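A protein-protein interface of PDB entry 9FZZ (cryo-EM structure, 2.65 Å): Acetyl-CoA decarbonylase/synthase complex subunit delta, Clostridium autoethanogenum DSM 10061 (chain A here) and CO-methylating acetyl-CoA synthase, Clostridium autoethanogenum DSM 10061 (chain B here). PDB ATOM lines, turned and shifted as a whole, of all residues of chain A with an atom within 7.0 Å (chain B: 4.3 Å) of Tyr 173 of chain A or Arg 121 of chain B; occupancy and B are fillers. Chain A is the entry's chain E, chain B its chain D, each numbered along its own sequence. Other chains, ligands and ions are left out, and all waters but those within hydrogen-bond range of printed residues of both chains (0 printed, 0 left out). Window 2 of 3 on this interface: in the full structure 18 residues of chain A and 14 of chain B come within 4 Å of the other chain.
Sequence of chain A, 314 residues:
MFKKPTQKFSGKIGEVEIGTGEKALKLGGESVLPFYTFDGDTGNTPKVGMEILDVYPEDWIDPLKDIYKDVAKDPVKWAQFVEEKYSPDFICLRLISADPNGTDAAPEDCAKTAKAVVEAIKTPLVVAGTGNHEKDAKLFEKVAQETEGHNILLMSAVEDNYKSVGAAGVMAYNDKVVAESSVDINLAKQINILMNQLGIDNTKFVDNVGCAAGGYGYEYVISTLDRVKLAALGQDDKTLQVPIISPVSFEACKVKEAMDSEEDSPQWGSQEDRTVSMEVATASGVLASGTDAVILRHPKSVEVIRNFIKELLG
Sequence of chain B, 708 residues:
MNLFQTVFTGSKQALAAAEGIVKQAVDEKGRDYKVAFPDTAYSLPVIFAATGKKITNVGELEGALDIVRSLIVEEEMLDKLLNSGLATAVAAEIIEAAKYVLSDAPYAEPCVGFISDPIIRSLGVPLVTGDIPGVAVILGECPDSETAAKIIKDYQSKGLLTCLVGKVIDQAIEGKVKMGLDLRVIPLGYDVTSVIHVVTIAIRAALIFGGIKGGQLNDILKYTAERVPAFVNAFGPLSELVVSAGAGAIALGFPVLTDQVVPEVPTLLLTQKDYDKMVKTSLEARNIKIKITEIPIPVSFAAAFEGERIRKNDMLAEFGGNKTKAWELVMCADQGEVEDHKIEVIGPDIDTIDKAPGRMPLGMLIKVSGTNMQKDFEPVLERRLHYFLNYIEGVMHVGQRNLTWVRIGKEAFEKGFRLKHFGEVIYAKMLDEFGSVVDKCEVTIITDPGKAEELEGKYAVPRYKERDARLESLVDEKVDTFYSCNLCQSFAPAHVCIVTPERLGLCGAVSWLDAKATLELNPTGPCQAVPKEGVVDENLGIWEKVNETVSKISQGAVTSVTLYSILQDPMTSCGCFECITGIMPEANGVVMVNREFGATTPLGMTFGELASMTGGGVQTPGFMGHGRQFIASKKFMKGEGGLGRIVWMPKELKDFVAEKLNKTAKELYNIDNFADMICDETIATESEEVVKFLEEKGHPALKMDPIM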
ATOM      1  N   PHE A 140       5.671  -6.628   2.191  1.00  0.00           N
ATOM      2  CA  PHE A 140       6.811  -6.160   2.971  1.00  0.00           C
ATOM      3  C   PHE A 140       8.038  -5.944   2.105  1.00  0.00           C
ATOM      4  O   PHE A 140       8.839  -5.053   2.390  1.00  0.00           O
ATOM      5  CB  PHE A 140       7.111  -7.132   4.111  1.00  0.00           C
ATOM      6  CG  PHE A 140       6.168  -7.005   5.275  1.00  0.00           C
ATOM      7  CD1 PHE A 140       5.786  -5.743   5.737  1.00  0.00           C
ATOM      8  CD2 PHE A 140       5.640  -8.130   5.888  1.00  0.00           C
ATOM      9  CE1 PHE A 140       4.902  -5.601   6.804  1.00  0.00           C
ATOM     10  CE2 PHE A 140       4.750  -8.011   6.958  1.00  0.00           C
ATOM     11  CZ  PHE A 140       4.379  -6.737   7.418  1.00  0.00           C
ATOM     12  N   GLU A 141       8.190  -6.722   1.037  1.00  0.00           N
ATOM     13  CA  GLU A 141       9.246  -6.438   0.072  1.00  0.00           C
ATOM     14  C   GLU A 141       9.138  -5.009  -0.442  1.00  0.00           C
ATOM     15  O   GLU A 141      10.079  -4.211  -0.330  1.00  0.00           O
ATOM     16  CB  GLU A 141       9.187  -7.431  -1.085  1.00  0.00           C
ATOM     17  CG  GLU A 141      10.152  -8.596  -0.907  1.00  0.00           C
ATOM     18  CD  GLU A 141       9.761  -9.802  -1.737  1.00  0.00           C
ATOM     19  OE1 GLU A 141       8.896  -9.654  -2.620  1.00  0.00           O
ATOM     20  OE2 GLU A 141      10.311 -10.898  -1.498  1.00  0.00           O
ATOM     21  N   VAL A 143       7.287  -2.525   0.764  1.00  0.00           N
ATOM     22  CA  VAL A 143       7.272  -1.542   1.848  1.00  0.00           C
ATOM     23  C   VAL A 143       8.683  -1.248   2.340  1.00  0.00           C
ATOM     24  O   VAL A 143       9.044  -0.090   2.567  1.00  0.00           O
ATOM     25  CB  VAL A 143       6.370  -2.016   2.999  1.00  0.00           C
ATOM     26  CG1 VAL A 143       6.607  -1.167   4.246  1.00  0.00           C
ATOM     27  CG2 VAL A 143       4.908  -1.933   2.599  1.00  0.00           C
ATOM     28  N   ALA A 144       9.502  -2.281   2.516  1.00  0.00           N
ATOM     29  CA  ALA A 144      10.874  -2.062   2.958  1.00  0.00           C
ATOM     30  C   ALA A 144      11.703  -1.414   1.865  1.00  0.00           C
ATOM     31  O   ALA A 144      12.619  -0.643   2.166  1.00  0.00           O
ATOM     32  CB  ALA A 144      11.507  -3.385   3.393  1.00  0.00           C
ATOM     33  N   GLN A 145      11.403  -1.701   0.598  1.00  0.00           N
ATOM     34  CA  GLN A 145      12.114  -1.011  -0.470  1.00  0.00           C
ATOM     35  C   GLN A 145      11.809   0.483  -0.456  1.00  0.00           C
ATOM     36  O   GLN A 145      12.719   1.307  -0.597  1.00  0.00           O
ATOM     37  CB  GLN A 145      11.755  -1.616  -1.826  1.00  0.00           C
ATOM     38  CG  GLN A 145      12.627  -1.087  -2.967  1.00  0.00           C
ATOM     39  CD  GLN A 145      11.910  -1.133  -4.308  1.00  0.00           C
ATOM     40  OE1 GLN A 145      12.109  -0.267  -5.157  1.00  0.00           O
ATOM     41  NE2 GLN A 145      11.061  -2.150  -4.500  1.00  0.00           N
ATOM     42  N   GLU A 146      10.537   0.860  -0.285  1.00  0.00           N
ATOM     43  CA  GLU A 146      10.187   2.282  -0.335  1.00  0.00           C
ATOM     44  C   GLU A 146      10.621   3.028   0.923  1.00  0.00           C
ATOM     45  O   GLU A 146      11.135   4.149   0.840  1.00  0.00           O
ATOM     46  CB  GLU A 146       8.682   2.441  -0.548  1.00  0.00           C
ATOM     47  CG  GLU A 146       8.228   2.068  -1.959  1.00  0.00           C
ATOM     48  CD  GLU A 146       8.404   3.208  -2.941  1.00  0.00           C
ATOM     49  OE1 GLU A 146       9.335   4.011  -2.755  1.00  0.00           O
ATOM     50  OE2 GLU A 146       7.599   3.307  -3.891  1.00  0.00           O
ATOM     51  N   THR A 147      10.419   2.435   2.098  1.00  0.00           N
ATOM     52  CA  THR A 147      10.739   3.086   3.374  1.00  0.00           C
ATOM     53  C   THR A 147      12.149   2.681   3.812  1.00  0.00           C
ATOM     54  O   THR A 147      12.360   1.947   4.779  1.00  0.00           O
ATOM     55  CB  THR A 147       9.711   2.727   4.436  1.00  0.00           C
ATOM     56  OG1 THR A 147       9.765   1.322   4.701  1.00  0.00           O
ATOM     57  CG2 THR A 147       8.327   3.094   3.973  1.00  0.00           C
ATOM     58  N   GLU A 148      13.130   3.191   3.075  1.00  0.00           N
ATOM     59  CA  GLU A 148      14.534   2.895   3.327  1.00  0.00           C
ATOM     60  C   GLU A 148      15.189   4.082   4.018  1.00  0.00           C
ATOM     61  O   GLU A 148      15.012   5.230   3.591  1.00  0.00           O
ATOM     62  CB  GLU A 148      15.271   2.576   2.027  1.00  0.00           C
ATOM     63  CG  GLU A 148      16.743   2.224   2.244  1.00  0.00           C
ATOM     64  CD  GLU A 148      17.468   1.962   0.939  1.00  0.00           C
ATOM     65  OE1 GLU A 148      16.859   2.195  -0.121  1.00  0.00           O
ATOM     66  OE2 GLU A 148      18.638   1.523   0.972  1.00  0.00           O
ATOM     67  N   GLY A 149      15.942   3.806   5.080  1.00  0.00           N
ATOM     68  CA  GLY A 149      16.645   4.835   5.810  1.00  0.00           C
ATOM     69  C   GLY A 149      15.951   5.353   7.050  1.00  0.00           C
ATOM     70  O   GLY A 149      16.398   6.363   7.606  1.00  0.00           O
ATOM     71  N   HIS A 150      14.883   4.695   7.511  1.00  0.00           N
ATOM     72  CA  HIS A 150      14.144   5.143   8.685  1.00  0.00           C
ATOM     73  C   HIS A 150      14.079   4.102   9.795  1.00  0.00           C
ATOM     74  O   HIS A 150      13.514   4.384  10.853  1.00  0.00           O
ATOM     75  CB  HIS A 150      12.725   5.561   8.285  1.00  0.00           C
ATOM     76  CG  HIS A 150      12.687   6.760   7.385  1.00  0.00           C
ATOM     77  ND1 HIS A 150      12.697   8.042   7.855  1.00  0.00           N
ATOM     78  CD2 HIS A 150      12.671   6.856   6.034  1.00  0.00           C
ATOM     79  CE1 HIS A 150      12.680   8.892   6.845  1.00  0.00           C
ATOM     80  NE2 HIS A 150      12.665   8.189   5.724  1.00  0.00           N
ATOM     81  N   ASN A 151      14.625   2.905   9.580  1.00  0.00           N
ATOM     82  CA  ASN A 151      14.712   1.880  10.620  1.00  0.00           C
ATOM     83  C   ASN A 151      13.334   1.530  11.179  1.00  0.00           C
ATOM     84  O   ASN A 151      13.095   1.570  12.387  1.00  0.00           O
ATOM     85  CB  ASN A 151      15.662   2.332  11.728  1.00  0.00           C
ATOM     86  CG  ASN A 151      16.051   1.209  12.675  1.00  0.00           C
ATOM     87  OD1 ASN A 151      15.925   0.041  12.333  1.00  0.00           O
ATOM     88  ND2 ASN A 151      16.526   1.557  13.866  1.00  0.00           N
ATOM     89  N   ILE A 152      12.421   1.158  10.284  1.00  0.00           N
ATOM     90  CA  ILE A 152      11.056   0.816  10.665  1.00  0.00           C
ATOM     91  C   ILE A 152      11.023  -0.618  11.181  1.00  0.00           C
ATOM     92  O   ILE A 152      12.012  -1.350  11.078  1.00  0.00           O
ATOM     93  CB  ILE A 152      10.072   1.002   9.497  1.00  0.00           C
ATOM     94  CG1 ILE A 152      10.287  -0.078   8.427  1.00  0.00           C
ATOM     95  CG2 ILE A 152      10.228   2.391   8.884  1.00  0.00           C
ATOM     96  CD1 ILE A 152       9.168  -0.141   7.431  1.00  0.00           C
ATOM     97  N   GLY A 166      12.772 -11.335   6.208  1.00  0.00           N
ATOM     98  CA  GLY A 166      14.111 -11.131   6.733  1.00  0.00           C
ATOM     99  C   GLY A 166      15.062 -10.554   5.702  1.00  0.00           C
ATOM    100  O   GLY A 166      15.853  -9.658   6.008  1.00  0.00           O
ATOM    101  N   ALA A 167      15.005 -11.059   4.469  1.00  0.00           N
ATOM    102  CA  ALA A 167      15.883 -10.552   3.420  1.00  0.00           C
ATOM    103  C   ALA A 167      15.490  -9.142   2.998  1.00  0.00           C
ATOM    104  O   ALA A 167      16.336  -8.244   2.935  1.00  0.00           O
ATOM    105  CB  ALA A 167      15.867 -11.504   2.221  1.00  0.00           C
ATOM    106  N   ALA A 168      14.205  -8.919   2.728  1.00  0.00           N
ATOM    107  CA  ALA A 168      13.752  -7.601   2.304  1.00  0.00           C
ATOM    108  C   ALA A 168      13.833  -6.584   3.430  1.00  0.00           C
ATOM    109  O   ALA A 168      13.826  -5.378   3.169  1.00  0.00           O
ATOM    110  CB  ALA A 168      12.319  -7.679   1.772  1.00  0.00           C
ATOM    111  N   GLY A 169      13.919  -7.050   4.665  1.00  0.00           N
ATOM    112  CA  GLY A 169      13.913  -6.214   5.843  1.00  0.00           C
ATOM    113  C   GLY A 169      15.321  -6.022   6.363  1.00  0.00           C
ATOM    114  O   GLY A 169      16.050  -5.140   5.901  1.00  0.00           O
ATOM    115  N   VAL A 170      15.707  -6.844   7.337  1.00  0.00           N
ATOM    116  CA  VAL A 170      16.984  -6.663   8.022  1.00  0.00           C
ATOM    117  C   VAL A 170      18.139  -6.647   7.029  1.00  0.00           C
ATOM    118  O   VAL A 170      18.987  -5.748   7.048  1.00  0.00           O
ATOM    119  CB  VAL A 170      17.183  -7.772   9.066  1.00  0.00           C
ATOM    120  CG1 VAL A 170      18.469  -7.534   9.845  1.00  0.00           C
ATOM    121  CG2 VAL A 170      15.982  -7.859  10.006  1.00  0.00           C
ATOM    122  N   MET A 171      18.176  -7.622   6.126  1.00  0.00           N
ATOM    123  CA  MET A 171      19.365  -7.829   5.304  1.00  0.00           C
ATOM    124  C   MET A 171      19.556  -6.713   4.281  1.00  0.00           C
ATOM    125  O   MET A 171      20.662  -6.175   4.137  1.00  0.00           O
ATOM    126  CB  MET A 171      19.283  -9.192   4.622  1.00  0.00           C
ATOM    127  CG  MET A 171      19.599 -10.354   5.559  1.00  0.00           C
ATOM    128  SD  MET A 171      19.497 -11.930   4.692  1.00  0.00           S
ATOM    129  CE  MET A 171      20.415 -13.003   5.775  1.00  0.00           C
ATOM    130  N   ALA A 172      18.502  -6.342   3.565  1.00  0.00           N
ATOM    131  CA  ALA A 172      18.640  -5.436   2.428  1.00  0.00           C
ATOM    132  C   ALA A 172      18.580  -3.971   2.850  1.00  0.00           C
ATOM    133  O   ALA A 172      19.513  -3.210   2.581  1.00  0.00           O
ATOM    134  CB  ALA A 172      17.561  -5.739   1.378  1.00  0.00           C
ATOM    135  N   TYR A 173      17.491  -3.554   3.504  1.00  0.00           N
ATOM    136  CA  TYR A 173      17.223  -2.143   3.741  1.00  0.00           C
ATOM    137  C   TYR A 173      17.378  -1.736   5.204  1.00  0.00           C
ATOM    138  O   TYR A 173      16.839  -0.708   5.623  1.00  0.00           O
ATOM    139  CB  TYR A 173      15.830  -1.778   3.226  1.00  0.00           C
ATOM    140  CG  TYR A 173      15.680  -2.081   1.756  1.00  0.00           C
ATOM    141  CD1 TYR A 173      16.232  -1.238   0.789  1.00  0.00           C
ATOM    142  CD2 TYR A 173      15.018  -3.229   1.328  1.00  0.00           C
ATOM    143  CE1 TYR A 173      16.113  -1.528  -0.576  1.00  0.00           C
ATOM    144  CE2 TYR A 173      14.889  -3.534  -0.025  1.00  0.00           C
ATOM    145  CZ  TYR A 173      15.438  -2.681  -0.966  1.00  0.00           C
ATOM    146  OH  TYR A 173      15.297  -3.006  -2.302  1.00  0.00           O
ATOM    147  N   ASN A 174      18.119  -2.518   5.990  1.00  0.00           N
ATOM    148  CA  ASN A 174      18.528  -2.123   7.338  1.00  0.00           C
ATOM    149  C   ASN A 174      17.334  -1.773   8.231  1.00  0.00           C
ATOM    150  O   ASN A 174      17.362  -0.797   8.981  1.00  0.00           O
ATOM    151  CB  ASN A 174      19.507  -0.949   7.287  1.00  0.00           C
ATOM    152  CG  ASN A 174      20.602  -1.138   6.243  1.00  0.00           C
ATOM    153  OD1 ASN A 174      21.194  -2.205   6.153  1.00  0.00           O
ATOM    154  ND2 ASN A 174      20.858  -0.104   5.439  1.00  0.00           N
ATOM    155  N   ASP A 175      16.277  -2.580   8.156  1.00  0.00           N
ATOM    156  CA  ASP A 175      15.110  -2.418   9.002  1.00  0.00           C
ATOM    157  C   ASP A 175      15.120  -3.481  10.096  1.00  0.00           C
ATOM    158  O   ASP A 175      16.002  -4.340  10.162  1.00  0.00           O
ATOM    159  CB  ASP A 175      13.826  -2.486   8.174  1.00  0.00           C
ATOM    160  CG  ASP A 175      13.674  -1.306   7.233  1.00  0.00           C
ATOM    161  OD1 ASP A 175      14.151  -0.209   7.585  1.00  0.00           O
ATOM    162  OD2 ASP A 175      13.089  -1.470   6.148  1.00  0.00           O
ATOM    163  N   LYS A 176      14.130  -3.412  10.978  1.00  0.00           N
ATOM    164  CA  LYS A 176      13.903  -4.421  12.000  1.00  0.00           C
ATOM    165  C   LYS A 176      12.659  -5.215  11.626  1.00  0.00           C
ATOM    166  O   LYS A 176      11.864  -4.793  10.785  1.00  0.00           O
ATOM    167  CB  LYS A 176      13.727  -3.783  13.383  1.00  0.00           C
ATOM    168  CG  LYS A 176      14.926  -2.940  13.823  1.00  0.00           C
ATOM    169  CD  LYS A 176      16.157  -3.828  14.031  1.00  0.00           C
ATOM    170  CE  LYS A 176      17.372  -3.010  14.473  1.00  0.00           C
ATOM    171  NZ  LYS A 176      17.800  -2.052  13.404  1.00  0.00           N
ATOM    172  N   ASP B 117      24.667  -0.876  -6.176  1.00  0.00           N
ATOM    173  CA  ASP B 117      24.152  -1.465  -4.944  1.00  0.00           C
ATOM    174  C   ASP B 117      22.636  -1.581  -4.895  1.00  0.00           C
ATOM    175  O   ASP B 117      22.138  -2.622  -4.432  1.00  0.00           O
ATOM    176  CB  ASP B 117      24.640  -0.662  -3.737  1.00  0.00           C
ATOM    177  CG  ASP B 117      25.956  -1.173  -3.179  1.00  0.00           C
ATOM    178  OD1 ASP B 117      26.193  -2.393  -3.261  1.00  0.00           O
ATOM    179  OD2 ASP B 117      26.746  -0.364  -2.662  1.00  0.00           O
ATOM    180  N   PRO B 118      21.850  -0.579  -5.305  1.00  0.00           N
ATOM    181  CA  PRO B 118      20.387  -0.764  -5.257  1.00  0.00           C
ATOM    182  C   PRO B 118      19.910  -1.948  -6.072  1.00  0.00           C
ATOM    183  O   PRO B 118      18.938  -2.606  -5.683  1.00  0.00           O
ATOM    184  CB  PRO B 118      19.847   0.567  -5.796  1.00  0.00           C
ATOM    185  CG  PRO B 118      20.952   1.580  -5.486  1.00  0.00           C
ATOM    186  CD  PRO B 118      22.236   0.798  -5.655  1.00  0.00           C
ATOM    187  N   ILE B 119      20.575  -2.259  -7.185  1.00  0.00           N
ATOM    188  CA  ILE B 119      20.200  -3.441  -7.954  1.00  0.00           C
ATOM    189  C   ILE B 119      20.453  -4.702  -7.139  1.00  0.00           C
ATOM    190  O   ILE B 119      19.628  -5.620  -7.117  1.00  0.00           O
ATOM    191  CB  ILE B 119      20.942  -3.461  -9.300  1.00  0.00           C
ATOM    192  CG1 ILE B 119      20.415  -2.319 -10.184  1.00  0.00           C
ATOM    193  CG2 ILE B 119      20.778  -4.819  -9.989  1.00  0.00           C
ATOM    194  CD1 ILE B 119      21.119  -2.199 -11.528  1.00  0.00           C
ATOM    195  N   ILE B 120      21.592  -4.761  -6.443  1.00  0.00           N
ATOM    196  CA  ILE B 120      21.900  -5.941  -5.639  1.00  0.00           C
ATOM    197  C   ILE B 120      20.849  -6.140  -4.556  1.00  0.00           C
ATOM    198  O   ILE B 120      20.379  -7.259  -4.322  1.00  0.00           O
ATOM    199  CB  ILE B 120      23.317  -5.840  -5.055  1.00  0.00           C
ATOM    200  CG1 ILE B 120      24.344  -5.911  -6.200  1.00  0.00           C
ATOM    201  CG2 ILE B 120      23.558  -6.946  -4.012  1.00  0.00           C
ATOM    202  CD1 ILE B 120      25.786  -5.984  -5.734  1.00  0.00           C
ATOM    203  N   ARG B 121      20.469  -5.062  -3.871  1.00  0.00           N
ATOM    204  CA  ARG B 121      19.403  -5.171  -2.879  1.00  0.00           C
ATOM    205  C   ARG B 121      18.075  -5.542  -3.526  1.00  0.00           C
ATOM    206  O   ARG B 121      17.245  -6.210  -2.901  1.00  0.00           O
ATOM    207  CB  ARG B 121      19.260  -3.855  -2.108  1.00  0.00           C
ATOM    208  CG  ARG B 121      20.546  -3.398  -1.431  1.00  0.00           C
ATOM    209  CD  ARG B 121      20.315  -2.099  -0.652  1.00  0.00           C
ATOM    210  NE  ARG B 121      21.571  -1.502  -0.215  1.00  0.00           N
ATOM    211  CZ  ARG B 121      22.180  -1.773   0.932  1.00  0.00           C
ATOM    212  NH1 ARG B 121      21.657  -2.603   1.818  1.00  0.00           N
ATOM    213  NH2 ARG B 121      23.354  -1.197   1.197  1.00  0.00           N
ATOM    214  N   SER B 122      17.860  -5.118  -4.774  1.00  0.00           N
ATOM    215  CA  SER B 122      16.635  -5.481  -5.479  1.00  0.00           C
ATOM    216  C   SER B 122      16.556  -6.977  -5.751  1.00  0.00           C
ATOM    217  O   SER B 122      15.507  -7.595  -5.537  1.00  0.00           O
ATOM    218  CB  SER B 122      16.560  -4.681  -6.786  1.00  0.00           C
ATOM    219  OG  SER B 122      15.404  -5.015  -7.543  1.00  0.00           O
ATOM    220  N   LEU B 123      17.646  -7.584  -6.210  1.00  0.00           N
ATOM    221  CA  LEU B 123      17.674  -9.015  -6.500  1.00  0.00           C
ATOM    222  C   LEU B 123      18.179  -9.853  -5.331  1.00  0.00           C
ATOM    223  O   LEU B 123      18.227 -11.081  -5.441  1.00  0.00           O
ATOM    224  CB  LEU B 123      18.510  -9.298  -7.758  1.00  0.00           C
ATOM    225  CG  LEU B 123      19.939  -8.741  -7.821  1.00  0.00           C
ATOM    226  CD1 LEU B 123      20.936  -9.623  -7.075  1.00  0.00           C
ATOM    227  CD2 LEU B 123      20.349  -8.568  -9.280  1.00  0.00           C
ATOM    228  N   GLY B 124      18.564  -9.219  -4.224  1.00  0.00           N
ATOM    229  CA  GLY B 124      19.021  -9.976  -3.072  1.00  0.00           C
ATOM    230  C   GLY B 124      17.918 -10.780  -2.409  1.00  0.00           C
ATOM    231  O   GLY B 124      18.145 -11.904  -1.958  1.00  0.00           O
ATOM    232  N   VAL B 125      16.719 -10.209  -2.322  1.00  0.00           N
ATOM    233  CA  VAL B 125      15.598 -10.933  -1.714  1.00  0.00           C
ATOM    234  C   VAL B 125      15.260 -12.195  -2.498  1.00  0.00           C
ATOM    235  O   VAL B 125      15.099 -13.258  -1.874  1.00  0.00           O
ATOM    236  CB  VAL B 125      14.390  -9.993  -1.537  1.00  0.00           C
ATOM    237  CG1 VAL B 125      13.364 -10.623  -0.594  1.00  0.00           C
ATOM    238  CG2 VAL B 125      14.836  -8.624  -1.006  1.00  0.00           C
ATOM    239  N   ILE B 208      26.580  -7.027   2.233  1.00  0.00           N
ATOM    240  CA  ILE B 208      25.270  -6.458   2.542  1.00  0.00           C
ATOM    241  C   ILE B 208      24.413  -7.422   3.345  1.00  0.00           C
ATOM    242  O   ILE B 208      23.889  -7.071   4.404  1.00  0.00           O
ATOM    243  CB  ILE B 208      24.565  -6.026   1.238  1.00  0.00           C
ATOM    244  CG1 ILE B 208      25.372  -4.915   0.552  1.00  0.00           C
ATOM    245  CG2 ILE B 208      23.137  -5.557   1.529  1.00  0.00           C
ATOM    246  CD1 ILE B 208      24.816  -4.480  -0.802  1.00  0.00           C
ATOM    247  N   PHE B 209      24.235  -8.648   2.853  1.00  0.00           N
ATOM    248  CA  PHE B 209      23.343  -9.597   3.505  1.00  0.00           C
ATOM    249  C   PHE B 209      24.046 -10.441   4.556  1.00  0.00           C
ATOM    250  O   PHE B 209      23.439 -10.773   5.578  1.00  0.00           O
ATOM    251  CB  PHE B 209      22.686 -10.502   2.458  1.00  0.00           C
ATOM    252  CG  PHE B 209      22.116  -9.747   1.285  1.00  0.00           C
ATOM    253  CD1 PHE B 209      20.999  -8.931   1.446  1.00  0.00           C
ATOM    254  CD2 PHE B 209      22.703  -9.833   0.032  1.00  0.00           C
ATOM    255  CE1 PHE B 209      20.463  -8.210   0.380  1.00  0.00           C
ATOM    256  CE2 PHE B 209      22.182  -9.116  -1.056  1.00  0.00           C
ATOM    257  CZ  PHE B 209      21.060  -8.296  -0.873  1.00  0.00           C
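O of Ile 208 of chain B sits close to O of Met 171 of chain A, at 3.4 Å.
O of Ala 172 of chain A lies close to NH1 of Arg 121 of chain B, at 2.4 Å.
The backbone NH (N) of Met 171 of chain A is in hydrogen-bond range of the backbone carbonyl oxygen (O) of Gly 166 of chain A, 3.1 Å away.
O of Ala 167 of chain A is in hydrogen-bond range of N of Ala 172 of chain A, at 3.0 Å.
Among the printed residues, merely in contact across the chains: Glu 141 of chain A with Val 125 of chain B (3.2 Å), Ala 167 of chain A with Val 125 of chain B (3.9 Å), Ala 168 of chain A with Val 125 of chain B (3.6 Å), Met 171 of chain A with Phe 209 of chain B (3.6 Å), Ala 172 of chain A with Phe 209 of chain B (3.9 Å) and Tyr 173 of chain A with Arg 121 of chain B (3.8 Å).
Of the printed residues of chain B, Ala 167 of chain A touches Val 125.
Of the printed residues of chain B, Met 171 of chain A touches Ile 208 and Phe 209.
Of the printed residues of chain B, Ala 172 of chain A touches Arg 121 (2.4 Å) and Phe 209 (3.9 Å).
Tyr 173 of chain A touches just one residue of chain B: Arg 121 (3.8 Å).
Of chain A, only Ala 172 and Tyr 173 come within 4 Å of Arg 121 of chain B.
Of the printed residues of chain A, Val 125 of chain B touches Glu 141, Ala 167 and Ala 168.
The nearest residue of chain B that does not touch Tyr 173 of chain A is Ser 122 of chain B (4.1 Å).
The nearest residue of chain A that does not touch Arg 121 of chain B is Glu 148 of chain A (4.3 Å).
The nearest printed residue of chain A that does not touch Val 125 of chain B is Ala 172 of chain A (4.6 Å).
Of the 23 printed residues of chain A, 6 touch a printed residue of chain B.
Printed residues of chain A that touch a printed residue of chain B: Glu 141, Ala 167, Ala 168, Met 171, Ala 172 and Tyr 173.
Printed residues of chain B that touch a printed residue of chain A: Arg 121, Val 125, Ile 208 and Phe 209.
Hydrophobic or aromatic side chains of chain B that line the printed part of chain A: Val 125, Ile 208 and Phe 209.
Along chain B the printed residues that touch a printed residue of chain A span positions 121 to 209.
Among the printed residues, 8 pairs touch across the chains.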
